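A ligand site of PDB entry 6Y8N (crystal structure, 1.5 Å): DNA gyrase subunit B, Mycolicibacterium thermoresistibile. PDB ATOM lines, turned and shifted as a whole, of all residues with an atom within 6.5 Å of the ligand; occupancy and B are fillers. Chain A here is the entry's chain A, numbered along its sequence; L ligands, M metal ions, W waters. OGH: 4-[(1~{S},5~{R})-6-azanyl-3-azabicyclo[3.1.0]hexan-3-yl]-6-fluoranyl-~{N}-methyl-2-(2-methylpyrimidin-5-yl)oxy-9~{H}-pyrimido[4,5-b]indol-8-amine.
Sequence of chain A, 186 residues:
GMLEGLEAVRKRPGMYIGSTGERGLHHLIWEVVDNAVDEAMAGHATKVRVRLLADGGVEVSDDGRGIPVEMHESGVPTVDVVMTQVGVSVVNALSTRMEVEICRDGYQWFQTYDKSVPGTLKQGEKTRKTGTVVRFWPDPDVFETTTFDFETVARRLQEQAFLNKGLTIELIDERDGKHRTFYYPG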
ATOM      1  N   GLU A  31      19.313 -16.297 -12.412  1.00  0.00           N
ATOM      2  CA  GLU A  31      19.230 -17.290 -11.317  1.00  0.00           C
ATOM      3  C   GLU A  31      20.372 -18.296 -11.534  1.00  0.00           C
ATOM      4  O   GLU A  31      21.024 -18.676 -10.563  1.00  0.00           O
ATOM      5  CB  GLU A  31      17.871 -17.995 -11.267  1.00  0.00           C
ATOM      6  CG  GLU A  31      17.611 -18.709  -9.933  1.00  0.00           C
ATOM      7  CD  GLU A  31      17.643 -17.821  -8.704  1.00  0.00           C
ATOM      8  OE1 GLU A  31      17.280 -16.622  -8.872  1.00  0.00           O
ATOM      9  OE2 GLU A  31      18.082 -18.297  -7.569  1.00  0.00           O
ATOM     10  N   VAL A  32      20.594 -18.717 -12.782  1.00  0.00           N
ATOM     11  CA  VAL A  32      21.584 -19.812 -12.998  1.00  0.00           C
ATOM     12  C   VAL A  32      22.985 -19.221 -12.841  1.00  0.00           C
ATOM     13  O   VAL A  32      23.844 -19.871 -12.216  1.00  0.00           O
ATOM     14  CB  VAL A  32      21.366 -20.511 -14.336  1.00  0.00           C
ATOM     15  CG1 VAL A  32      22.430 -21.588 -14.554  1.00  0.00           C
ATOM     16  CG2 VAL A  32      19.970 -21.108 -14.413  1.00  0.00           C
ATOM     17  N   VAL A  33      23.198 -18.041 -13.386  1.00  0.00           N
ATOM     18  CA  VAL A  33      24.497 -17.320 -13.214  1.00  0.00           C
ATOM     19  C   VAL A  33      24.758 -17.132 -11.718  1.00  0.00           C
ATOM     20  O   VAL A  33      25.917 -17.345 -11.266  1.00  0.00           O
ATOM     21  CB  VAL A  33      24.524 -15.986 -13.969  1.00  0.00           C
ATOM     22  CG1 VAL A  33      25.643 -15.088 -13.484  1.00  0.00           C
ATOM     23  CG2 VAL A  33      24.630 -16.216 -15.468  1.00  0.00           C
ATOM     24  N   ASN A  35      23.861 -18.845  -9.105  1.00  0.00           N
ATOM     25  CA  ASN A  35      24.265 -20.120  -8.449  1.00  0.00           C
ATOM     26  C   ASN A  35      25.703 -20.476  -8.824  1.00  0.00           C
ATOM     27  O   ASN A  35      26.422 -20.964  -7.976  1.00  0.00           O
ATOM     28  CB  ASN A  35      23.299 -21.243  -8.786  1.00  0.00           C
ATOM     29  CG  ASN A  35      22.081 -21.148  -7.903  1.00  0.00           C
ATOM     30  OD1 ASN A  35      22.145 -21.449  -6.709  1.00  0.00           O
ATOM     31  ND2 ASN A  35      21.006 -20.621  -8.434  1.00  0.00           N
ATOM     32  N   ALA A  36      26.103 -20.234 -10.054  1.00  0.00           N
ATOM     33  CA  ALA A  36      27.485 -20.501 -10.496  1.00  0.00           C
ATOM     34  C   ALA A  36      28.442 -19.562  -9.748  1.00  0.00           C
ATOM     35  O   ALA A  36      29.497 -19.992  -9.256  1.00  0.00           O
ATOM     36  CB  ALA A  36      27.599 -20.315 -11.990  1.00  0.00           C
ATOM     37  N   VAL A  37      28.116 -18.286  -9.687  1.00  0.00           N
ATOM     38  CA  VAL A  37      29.014 -17.285  -9.075  1.00  0.00           C
ATOM     39  C   VAL A  37      29.076 -17.555  -7.574  1.00  0.00           C
ATOM     40  O   VAL A  37      30.167 -17.338  -7.001  1.00  0.00           O
ATOM     41  CB  VAL A  37      28.564 -15.853  -9.418  1.00  0.00           C
ATOM     42  CG1 VAL A  37      29.365 -14.844  -8.635  1.00  0.00           C
ATOM     43  CG2 VAL A  37      28.700 -15.606 -10.898  1.00  0.00           C
ATOM     44  N   ASP A  38      27.977 -17.968  -6.950  1.00  0.00           N
ATOM     45  CA  ASP A  38      27.954 -18.327  -5.508  1.00  0.00           C
ATOM     46  C   ASP A  38      29.081 -19.323  -5.201  1.00  0.00           C
ATOM     47  O   ASP A  38      29.609 -19.305  -4.066  1.00  0.00           O
ATOM     48  CB  ASP A  38      26.619 -18.910  -5.081  1.00  0.00           C
ATOM     49  CG  ASP A  38      25.473 -17.918  -4.915  1.00  0.00           C
ATOM     50  OD1 ASP A  38      25.729 -16.686  -4.917  1.00  0.00           O
ATOM     51  OD2 ASP A  38      24.337 -18.402  -4.771  1.00  0.00           O
ATOM     52  N   GLU A  39      29.426 -20.188  -6.144  1.00  0.00           N
ATOM     53  CA  GLU A  39      30.502 -21.216  -5.964  1.00  0.00           C
ATOM     54  C   GLU A  39      31.872 -20.554  -5.878  1.00  0.00           C
ATOM     55  O   GLU A  39      32.782 -21.233  -5.375  1.00  0.00           O
ATOM     56  CB  GLU A  39      30.538 -22.230  -7.106  1.00  0.00           C
ATOM     57  CG  GLU A  39      29.588 -23.344  -6.955  1.00  0.00           C
ATOM     58  CD  GLU A  39      29.637 -24.001  -5.592  1.00  0.00           C
ATOM     59  OE1 GLU A  39      30.592 -24.767  -5.313  1.00  0.00           O
ATOM     60  OE2 GLU A  39      28.688 -23.724  -4.824  1.00  0.00           O
ATOM     61  N   ALA A  42      32.037 -19.786  -2.153  1.00  0.00           N
ATOM     62  CA  ALA A  42      31.564 -20.913  -1.300  1.00  0.00           C
ATOM     63  C   ALA A  42      32.213 -22.239  -1.684  1.00  0.00           C
ATOM     64  O   ALA A  42      32.230 -23.188  -0.848  1.00  0.00           O
ATOM     65  CB  ALA A  42      30.052 -21.038  -1.389  1.00  0.00           C
ATOM     66  N   GLY A  43      32.645 -22.392  -2.930  1.00  0.00           N
ATOM     67  CA  GLY A  43      33.081 -23.692  -3.479  1.00  0.00           C
ATOM     68  C   GLY A  43      34.406 -23.651  -4.203  1.00  0.00           C
ATOM     69  O   GLY A  43      34.719 -24.632  -4.910  1.00  0.00           O
ATOM     70  N   VAL A  48      33.739 -19.175 -14.289  1.00  0.00           N
ATOM     71  CA  VAL A  48      32.333 -19.352 -14.719  1.00  0.00           C
ATOM     72  C   VAL A  48      32.288 -19.060 -16.212  1.00  0.00           C
ATOM     73  O   VAL A  48      32.880 -18.062 -16.647  1.00  0.00           O
ATOM     74  CB  VAL A  48      31.409 -18.399 -13.945  1.00  0.00           C
ATOM     75  CG1 VAL A  48      30.006 -18.392 -14.533  1.00  0.00           C
ATOM     76  CG2 VAL A  48      31.366 -18.742 -12.455  1.00  0.00           C
ATOM     77  N   ARG A  49      31.571 -19.892 -16.968  1.00  0.00           N
ATOM     78  CA  ARG A  49      31.370 -19.652 -18.404  1.00  0.00           C
ATOM     79  C   ARG A  49      29.879 -19.597 -18.681  1.00  0.00           C
ATOM     80  O   ARG A  49      29.128 -20.434 -18.175  1.00  0.00           O
ATOM     81  CB  ARG A  49      32.056 -20.731 -19.243  1.00  0.00           C
ATOM     82  CG  ARG A  49      31.917 -20.516 -20.740  1.00  0.00           C
ATOM     83  CD  ARG A  49      32.474 -21.720 -21.484  1.00  0.00           C
ATOM     84  NE  ARG A  49      33.912 -21.621 -21.537  1.00  0.00           N
ATOM     85  CZ  ARG A  49      34.714 -22.438 -22.200  1.00  0.00           C
ATOM     86  NH1 ARG A  49      34.212 -23.486 -22.859  1.00  0.00           N
ATOM     87  NH2 ARG A  49      36.016 -22.227 -22.195  1.00  0.00           N
ATOM     88  N   VAL A  60      25.420 -22.528 -18.575  1.00  0.00           N
ATOM     89  CA  VAL A  60      26.274 -21.912 -17.545  1.00  0.00           C
ATOM     90  C   VAL A  60      27.084 -23.025 -16.891  1.00  0.00           C
ATOM     91  O   VAL A  60      26.522 -24.036 -16.532  1.00  0.00           O
ATOM     92  CB  VAL A  60      25.424 -21.191 -16.500  1.00  0.00           C
ATOM     93  CG1 VAL A  60      26.343 -20.497 -15.513  1.00  0.00           C
ATOM     94  CG2 VAL A  60      24.461 -20.246 -17.192  1.00  0.00           C
ATOM     95  N   SER A  61      28.372 -22.778 -16.713  1.00  0.00           N
ATOM     96  CA  SER A  61      29.264 -23.773 -16.088  1.00  0.00           C
ATOM     97  C   SER A  61      30.156 -23.108 -15.046  1.00  0.00           C
ATOM     98  O   SER A  61      30.508 -21.944 -15.186  1.00  0.00           O
ATOM     99  CB  SER A  61      30.054 -24.511 -17.115  1.00  0.00           C
ATOM    100  OG  SER A  61      30.822 -23.613 -17.853  1.00  0.00           O
ATOM    101  N   ASP A  62      30.524 -23.895 -14.054  1.00  0.00           N
ATOM    102  CA  ASP A  62      31.503 -23.461 -13.053  1.00  0.00           C
ATOM    103  C   ASP A  62      32.420 -24.642 -12.745  1.00  0.00           C
ATOM    104  O   ASP A  62      32.047 -25.804 -12.994  1.00  0.00           O
ATOM    105  CB  ASP A  62      30.843 -22.908 -11.795  1.00  0.00           C
ATOM    106  CG  ASP A  62      30.095 -23.946 -10.979  1.00  0.00           C
ATOM    107  OD1 ASP A  62      30.743 -24.808 -10.399  1.00  0.00           O
ATOM    108  OD2 ASP A  62      28.886 -23.824 -10.892  1.00  0.00           O
ATOM    109  N   GLY A  64      33.295 -25.324  -9.587  1.00  0.00           N
ATOM    110  CA  GLY A  64      33.090 -25.439  -8.140  1.00  0.00           C
ATOM    111  C   GLY A  64      32.977 -26.865  -7.647  1.00  0.00           C
ATOM    112  O   GLY A  64      33.566 -27.796  -8.241  1.00  0.00           O
ATOM    113  N   ARG A  65      32.236 -27.038  -6.559  1.00  0.00           N
ATOM    114  CA  ARG A  65      32.104 -28.324  -5.837  1.00  0.00           C
ATOM    115  C   ARG A  65      31.275 -29.352  -6.636  1.00  0.00           C
ATOM    116  O   ARG A  65      31.425 -30.548  -6.386  1.00  0.00           O
ATOM    117  CB  ARG A  65      31.417 -28.077  -4.492  1.00  0.00           C
ATOM    118  CG  ARG A  65      32.289 -27.331  -3.493  1.00  0.00           C
ATOM    119  CD  ARG A  65      31.512 -26.826  -2.285  1.00  0.00           C
ATOM    120  NE  ARG A  65      30.580 -25.763  -2.624  1.00  0.00           N
ATOM    121  CZ  ARG A  65      29.760 -25.139  -1.771  1.00  0.00           C
ATOM    122  NH1 ARG A  65      29.674 -25.551  -0.524  1.00  0.00           N
ATOM    123  NH2 ARG A  65      28.950 -24.167  -2.193  1.00  0.00           N
ATOM    124  N   GLY A  66      30.415 -28.895  -7.531  1.00  0.00           N
ATOM    125  CA  GLY A  66      29.410 -29.763  -8.173  1.00  0.00           C
ATOM    126  C   GLY A  66      28.161 -29.862  -7.309  1.00  0.00           C
ATOM    127  O   GLY A  66      28.261 -30.133  -6.095  1.00  0.00           O
ATOM    128  N   ILE A  67      27.003 -29.670  -7.925  1.00  0.00           N
ATOM    129  CA  ILE A  67      25.702 -29.862  -7.223  1.00  0.00           C
ATOM    130  C   ILE A  67      25.728 -31.243  -6.574  1.00  0.00           C
ATOM    131  O   ILE A  67      26.025 -32.238  -7.235  1.00  0.00           O
ATOM    132  CB  ILE A  67      24.484 -29.736  -8.141  1.00  0.00           C
ATOM    133  CG1 ILE A  67      24.412 -28.390  -8.850  1.00  0.00           C
ATOM    134  CG2 ILE A  67      23.227 -29.958  -7.310  1.00  0.00           C
ATOM    135  CD1 ILE A  67      23.339 -28.330  -9.915  1.00  0.00           C
ATOM    136  N   PRO A  68      25.422 -31.353  -5.270  1.00  0.00           N
ATOM    137  CA  PRO A  68      25.392 -32.671  -4.645  1.00  0.00           C
ATOM    138  C   PRO A  68      24.493 -33.668  -5.382  1.00  0.00           C
ATOM    139  O   PRO A  68      23.377 -33.336  -5.792  1.00  0.00           O
ATOM    140  CB  PRO A  68      24.866 -32.368  -3.235  1.00  0.00           C
ATOM    141  CG  PRO A  68      25.387 -30.970  -2.993  1.00  0.00           C
ATOM    142  CD  PRO A  68      25.173 -30.258  -4.312  1.00  0.00           C
ATOM    143  N   THR A  78      19.986 -35.256  -4.465  1.00  0.00           N
ATOM    144  CA  THR A  78      19.894 -33.843  -4.023  1.00  0.00           C
ATOM    145  C   THR A  78      19.717 -32.929  -5.237  1.00  0.00           C
ATOM    146  O   THR A  78      18.969 -31.941  -5.156  1.00  0.00           O
ATOM    147  CB  THR A  78      21.105 -33.460  -3.162  1.00  0.00           C
ATOM    148  OG1 THR A  78      21.065 -34.288  -1.996  1.00  0.00           O
ATOM    149  CG2 THR A  78      21.058 -31.993  -2.780  1.00  0.00           C
ATOM    150  N   VAL A  82      17.178 -29.714  -5.638  1.00  0.00           N
ATOM    151  CA  VAL A  82      17.626 -28.354  -6.057  1.00  0.00           C
ATOM    152  C   VAL A  82      16.751 -27.887  -7.233  1.00  0.00           C
ATOM    153  O   VAL A  82      16.179 -26.736  -7.201  1.00  0.00           O
ATOM    154  CB  VAL A  82      19.105 -28.352  -6.419  1.00  0.00           C
ATOM    155  CG1 VAL A  82      19.509 -27.088  -7.126  1.00  0.00           C
ATOM    156  CG2 VAL A  82      19.987 -28.608  -5.221  1.00  0.00           C
ATOM    157  N   MET A  83      16.572 -28.746  -8.223  1.00  0.00           N
ATOM    158  CA  MET A  83      15.942 -28.304  -9.485  1.00  0.00           C
ATOM    159  C   MET A  83      14.414 -28.303  -9.343  1.00  0.00           C
ATOM    160  O   MET A  83      13.747 -27.861 -10.296  1.00  0.00           O
ATOM    161  CB  MET A  83      16.391 -29.195 -10.641  1.00  0.00           C
ATOM    162  CG  MET A  83      17.823 -28.943 -11.042  1.00  0.00           C
ATOM    163  SD  MET A  83      18.150 -27.197 -11.315  1.00  0.00           S
ATOM    164  CE  MET A  83      19.942 -27.238 -11.500  1.00  0.00           C
ATOM    165  N   VAL A  86      14.540 -25.174  -4.940  1.00  0.00           N
ATOM    166  CA  VAL A  86      15.336 -23.973  -4.723  1.00  0.00           C
ATOM    167  C   VAL A  86      15.011 -22.925  -5.815  1.00  0.00           C
ATOM    168  O   VAL A  86      14.220 -23.224  -6.701  1.00  0.00           O
ATOM    169  CB  VAL A  86      16.819 -24.426  -4.662  1.00  0.00           C
ATOM    170  CG1 VAL A  86      17.837 -23.316  -4.748  1.00  0.00           C
ATOM    171  CG2 VAL A  86      17.058 -25.263  -3.410  1.00  0.00           C
ATOM    172  N   VAL A  88      16.375 -21.894  -8.466  1.00  0.00           N
ATOM    173  CA  VAL A  88      16.657 -22.311  -9.864  1.00  0.00           C
ATOM    174  C   VAL A  88      15.534 -23.228 -10.362  1.00  0.00           C
ATOM    175  O   VAL A  88      15.426 -23.407 -11.592  1.00  0.00           O
ATOM    176  CB  VAL A  88      18.077 -22.925  -9.957  1.00  0.00           C
ATOM    177  CG1 VAL A  88      18.180 -24.250  -9.222  1.00  0.00           C
ATOM    178  CG2 VAL A  88      18.576 -23.026 -11.373  1.00  0.00           C
ATOM    179  N   MET A  98      15.857 -29.029 -19.364  1.00  0.00           N
ATOM    180  CA  MET A  98      17.140 -28.642 -18.747  1.00  0.00           C
ATOM    181  C   MET A  98      18.039 -29.877 -18.763  1.00  0.00           C
ATOM    182  O   MET A  98      17.518 -30.989 -18.588  1.00  0.00           O
ATOM    183  CB  MET A  98      16.985 -28.216 -17.289  1.00  0.00           C
ATOM    184  CG  MET A  98      16.119 -27.052 -17.090  1.00  0.00           C
ATOM    185  SD  MET A  98      16.462 -26.228 -15.483  1.00  0.00           S
ATOM    186  CE  MET A  98      17.659 -27.282 -14.672  1.00  0.00           C
ATOM    187  N   ARG A 104      31.809 -34.580  -9.572  1.00  0.00           N
ATOM    188  CA  ARG A 104      32.116 -34.626  -8.123  1.00  0.00           C
ATOM    189  C   ARG A 104      32.210 -36.071  -7.658  1.00  0.00           C
ATOM    190  O   ARG A 104      31.667 -36.984  -8.339  1.00  0.00           O
ATOM    191  CB  ARG A 104      31.050 -33.885  -7.341  1.00  0.00           C
ATOM    192  CG  ARG A 104      29.687 -34.544  -7.284  1.00  0.00           C
ATOM    193  CD  ARG A 104      28.851 -33.690  -6.316  1.00  0.00           C
ATOM    194  NE  ARG A 104      29.233 -33.992  -4.962  1.00  0.00           N
ATOM    195  CZ  ARG A 104      29.537 -33.131  -3.988  1.00  0.00           C
ATOM    196  NH1 ARG A 104      29.497 -31.831  -4.172  1.00  0.00           N
ATOM    197  NH2 ARG A 104      29.889 -33.615  -2.805  1.00  0.00           N
ATOM    198  N   GLY A 131      32.740 -29.642 -10.706  1.00  0.00           N
ATOM    199  CA  GLY A 131      31.977 -28.465 -11.163  1.00  0.00           C
ATOM    200  C   GLY A 131      30.616 -28.859 -11.656  1.00  0.00           C
ATOM    201  O   GLY A 131      30.218 -30.022 -11.498  1.00  0.00           O
ATOM    202  N   THR A 132      29.924 -27.893 -12.201  1.00  0.00           N
ATOM    203  CA  THR A 132      28.515 -28.028 -12.611  1.00  0.00           C
ATOM    204  C   THR A 132      28.336 -27.331 -13.961  1.00  0.00           C
ATOM    205  O   THR A 132      28.887 -26.258 -14.168  1.00  0.00           O
ATOM    206  CB  THR A 132      27.585 -27.343 -11.601  1.00  0.00           C
ATOM    207  OG1 THR A 132      27.737 -27.961 -10.326  1.00  0.00           O
ATOM    208  CG2 THR A 132      26.134 -27.436 -11.987  1.00  0.00           C
ATOM    209  N   VAL A 133      27.569 -27.956 -14.828  1.00  0.00           N
ATOM    210  CA  VAL A 133      27.095 -27.352 -16.097  1.00  0.00           C
ATOM    211  C   VAL A 133      25.575 -27.453 -16.091  1.00  0.00           C
ATOM    212  O   VAL A 133      25.051 -28.561 -15.869  1.00  0.00           O
ATOM    213  CB  VAL A 133      27.679 -28.065 -17.324  1.00  0.00           C
ATOM    214  CG1 VAL A 133      27.254 -27.379 -18.585  1.00  0.00           C
ATOM    215  CG2 VAL A 133      29.191 -28.189 -17.269  1.00  0.00           C
ATOM    216  N   VAL A 134      24.911 -26.334 -16.317  1.00  0.00           N
ATOM    217  CA  VAL A 134      23.427 -26.342 -16.471  1.00  0.00           C
ATOM    218  C   VAL A 134      23.084 -25.731 -17.828  1.00  0.00           C
ATOM    219  O   VAL A 134      23.597 -24.655 -18.157  1.00  0.00           O
ATOM    220  CB  VAL A 134      22.725 -25.589 -15.326  1.00  0.00           C
ATOM    221  CG1 VAL A 134      21.220 -25.478 -15.549  1.00  0.00           C
ATOM    222  CG2 VAL A 134      23.006 -26.278 -14.007  1.00  0.00           C
HETATM  223  N1  OGH L   1      26.651 -26.470  -1.957  1.00  0.00           N
HETATM  224  N3  OGH L   1      27.481 -25.611  -7.305  1.00  0.00           N
HETATM  225  C4  OGH L   1      27.633 -26.987  -4.056  1.00  0.00           C
HETATM  226  C5  OGH L   1      28.101 -28.156  -3.509  1.00  0.00           C
HETATM  227  C6  OGH L   1      27.039 -26.163  -6.185  1.00  0.00           C
HETATM  228  C7  OGH L   1      26.532 -25.183  -8.144  1.00  0.00           C
HETATM  229  C8  OGH L   1      25.143 -25.186  -7.861  1.00  0.00           C
HETATM  230  C10 OGH L   1      23.152 -24.565  -9.496  1.00  0.00           C
HETATM  231  C13 OGH L   1      25.271 -23.917 -11.226  1.00  0.00           C
HETATM  232  C15 OGH L   1      26.254 -23.507 -13.481  1.00  0.00           C
HETATM  233  C17 OGH L   1      23.088 -26.488  -4.944  1.00  0.00           C
HETATM  234  C20 OGH L   1      22.595 -24.666  -6.444  1.00  0.00           C
HETATM  235  C21 OGH L   1      23.336 -24.113  -4.044  1.00  0.00           C
HETATM  236  C1  OGH L   1      26.889 -27.992  -0.070  1.00  0.00           C
HETATM  237  C2  OGH L   1      27.153 -27.615  -1.488  1.00  0.00           C
HETATM  238  C3  OGH L   1      26.907 -26.146  -3.228  1.00  0.00           C
HETATM  239  N2  OGH L   1      27.873 -28.463  -2.221  1.00  0.00           N
HETATM  240  O1  OGH L   1      27.970 -26.679  -5.375  1.00  0.00           O
HETATM  241  C9  OGH L   1      24.479 -24.685  -9.042  1.00  0.00           C
HETATM  242  C11 OGH L   1      22.942 -24.171 -10.803  1.00  0.00           C
HETATM  243  C12 OGH L   1      23.961 -23.798 -11.642  1.00  0.00           C
HETATM  244  C14 OGH L   1      25.522 -24.369  -9.948  1.00  0.00           C
HETATM  245  N4  OGH L   1      26.735 -24.635  -9.351  1.00  0.00           N
HETATM  246  N5  OGH L   1      26.346 -23.623 -12.047  1.00  0.00           N
HETATM  247  F1  OGH L   1      21.659 -24.039 -11.279  1.00  0.00           F
HETATM  248  C16 OGH L   1      24.787 -25.747  -6.601  1.00  0.00           C
HETATM  249  N6  OGH L   1      25.765 -26.231  -5.799  1.00  0.00           N
HETATM  250  N7  OGH L   1      23.531 -25.739  -6.114  1.00  0.00           N
HETATM  251  C18 OGH L   1      22.514 -25.375  -4.104  1.00  0.00           C
HETATM  252  C19 OGH L   1      22.195 -24.240  -5.048  1.00  0.00           C
HETATM  253  N8  OGH L   1      23.146 -23.241  -2.904  1.00  0.00           N
HETATM  254 ZN    ZN M   1      22.944 -17.097  -4.928  1.00  0.00          ZN
HETATM  255  O   HOH W   1      29.161 -30.500  -0.988  1.00  0.00           O
HETATM  256  O   HOH W   2      24.784 -24.626  -1.092  1.00  0.00           O
HETATM  257  O   HOH W   3      21.430 -20.976  -4.313  1.00  0.00           O
HETATM  258  O   HOH W   4      24.138 -21.115  -4.379  1.00  0.00           O
HETATM  259  O   HOH W   5      29.577 -26.563  -8.900  1.00  0.00           O
HETATM  260  O   HOH W   6      26.024 -22.595  -5.745  1.00  0.00           O
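OD2 of Asp 62 lies within hydrogen-bond range of N4 of the ligand.
The side-chain carboxylate (OE2) of Glu 39 lies close to a nitrogen (N3) of the ligand, 3.3 Å away.
N1 of the ligand sits close to NH2 of Arg 65.
O of Arg 65 is in hydrogen-bond range of NH1 of Arg 104 (3.2 Å).
The backbone carbonyl oxygen (O) of Val 60 is in hydrogen-bond range of the backbone NH (N) of Val 134, 2.8 Å away.
N of Asp 62 sits at hydrogen-bond distance from O of Thr 132 (2.9 Å).
The backbone carbonyl oxygen of Gly 66 lies within hydrogen-bond range of the guanidinium group of Arg 104, at 2.8 Å.
The backbone NH of Ser 61 sits at hydrogen-bond distance from the backbone carbonyl oxygen of Arg 49 (2.9 Å).
The backbone carbonyl oxygen of Ala 42 sits close to the guanidinium group of Arg 65.
ND2 of Asn 35 lies within hydrogen-bond range of O of Glu 31 (2.9 Å).
The side-chain hydroxyl of Thr 132 sits at hydrogen-bond distance from the backbone NH of Ile 67, at 3.0 Å.
Merely in contact with the ligand: Val 32, Asn 35, Ala 36, Val 60, Ser 61, Gly 66, Ile 67, Pro 68, Val 82, Met 83, Val 88, Arg 104, Thr 132 and Val 134.
Hydrophobic or aromatic side chains that line the ligand: Val 32, Ala 36, Val 60, Ile 67, Pro 68, Val 82, Met 83, Val 88 and Val 134.
Water W1 bridges N2 of the ligand (2.7 Å) and NH1 of Arg 104 (3.5 Å).
Water W4 bridges N8 of the ligand and OD1 of Asn 35.
Water W5 lies within hydrogen-bond range of the side-chain carboxylate of Asp 62 (2.6 Å), the side-chain hydroxyl of Thr 132 (2.7 Å), a nitrogen (N3) of the ligand (2.8 Å) and the backbone NH of Gly 66 (2.8 Å).
Water W3 lies within hydrogen-bond range of the side-chain amide oxygen of Asn 35 (2.5 Å) and a nitrogen (N8) of the ligand (3.2 Å).
Water W6 lies within hydrogen-bond range of the backbone carbonyl oxygen (O) of Asn 35 (2.8 Å) and the side-chain carboxylate (OE2) of Glu 39 (3.0 Å).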
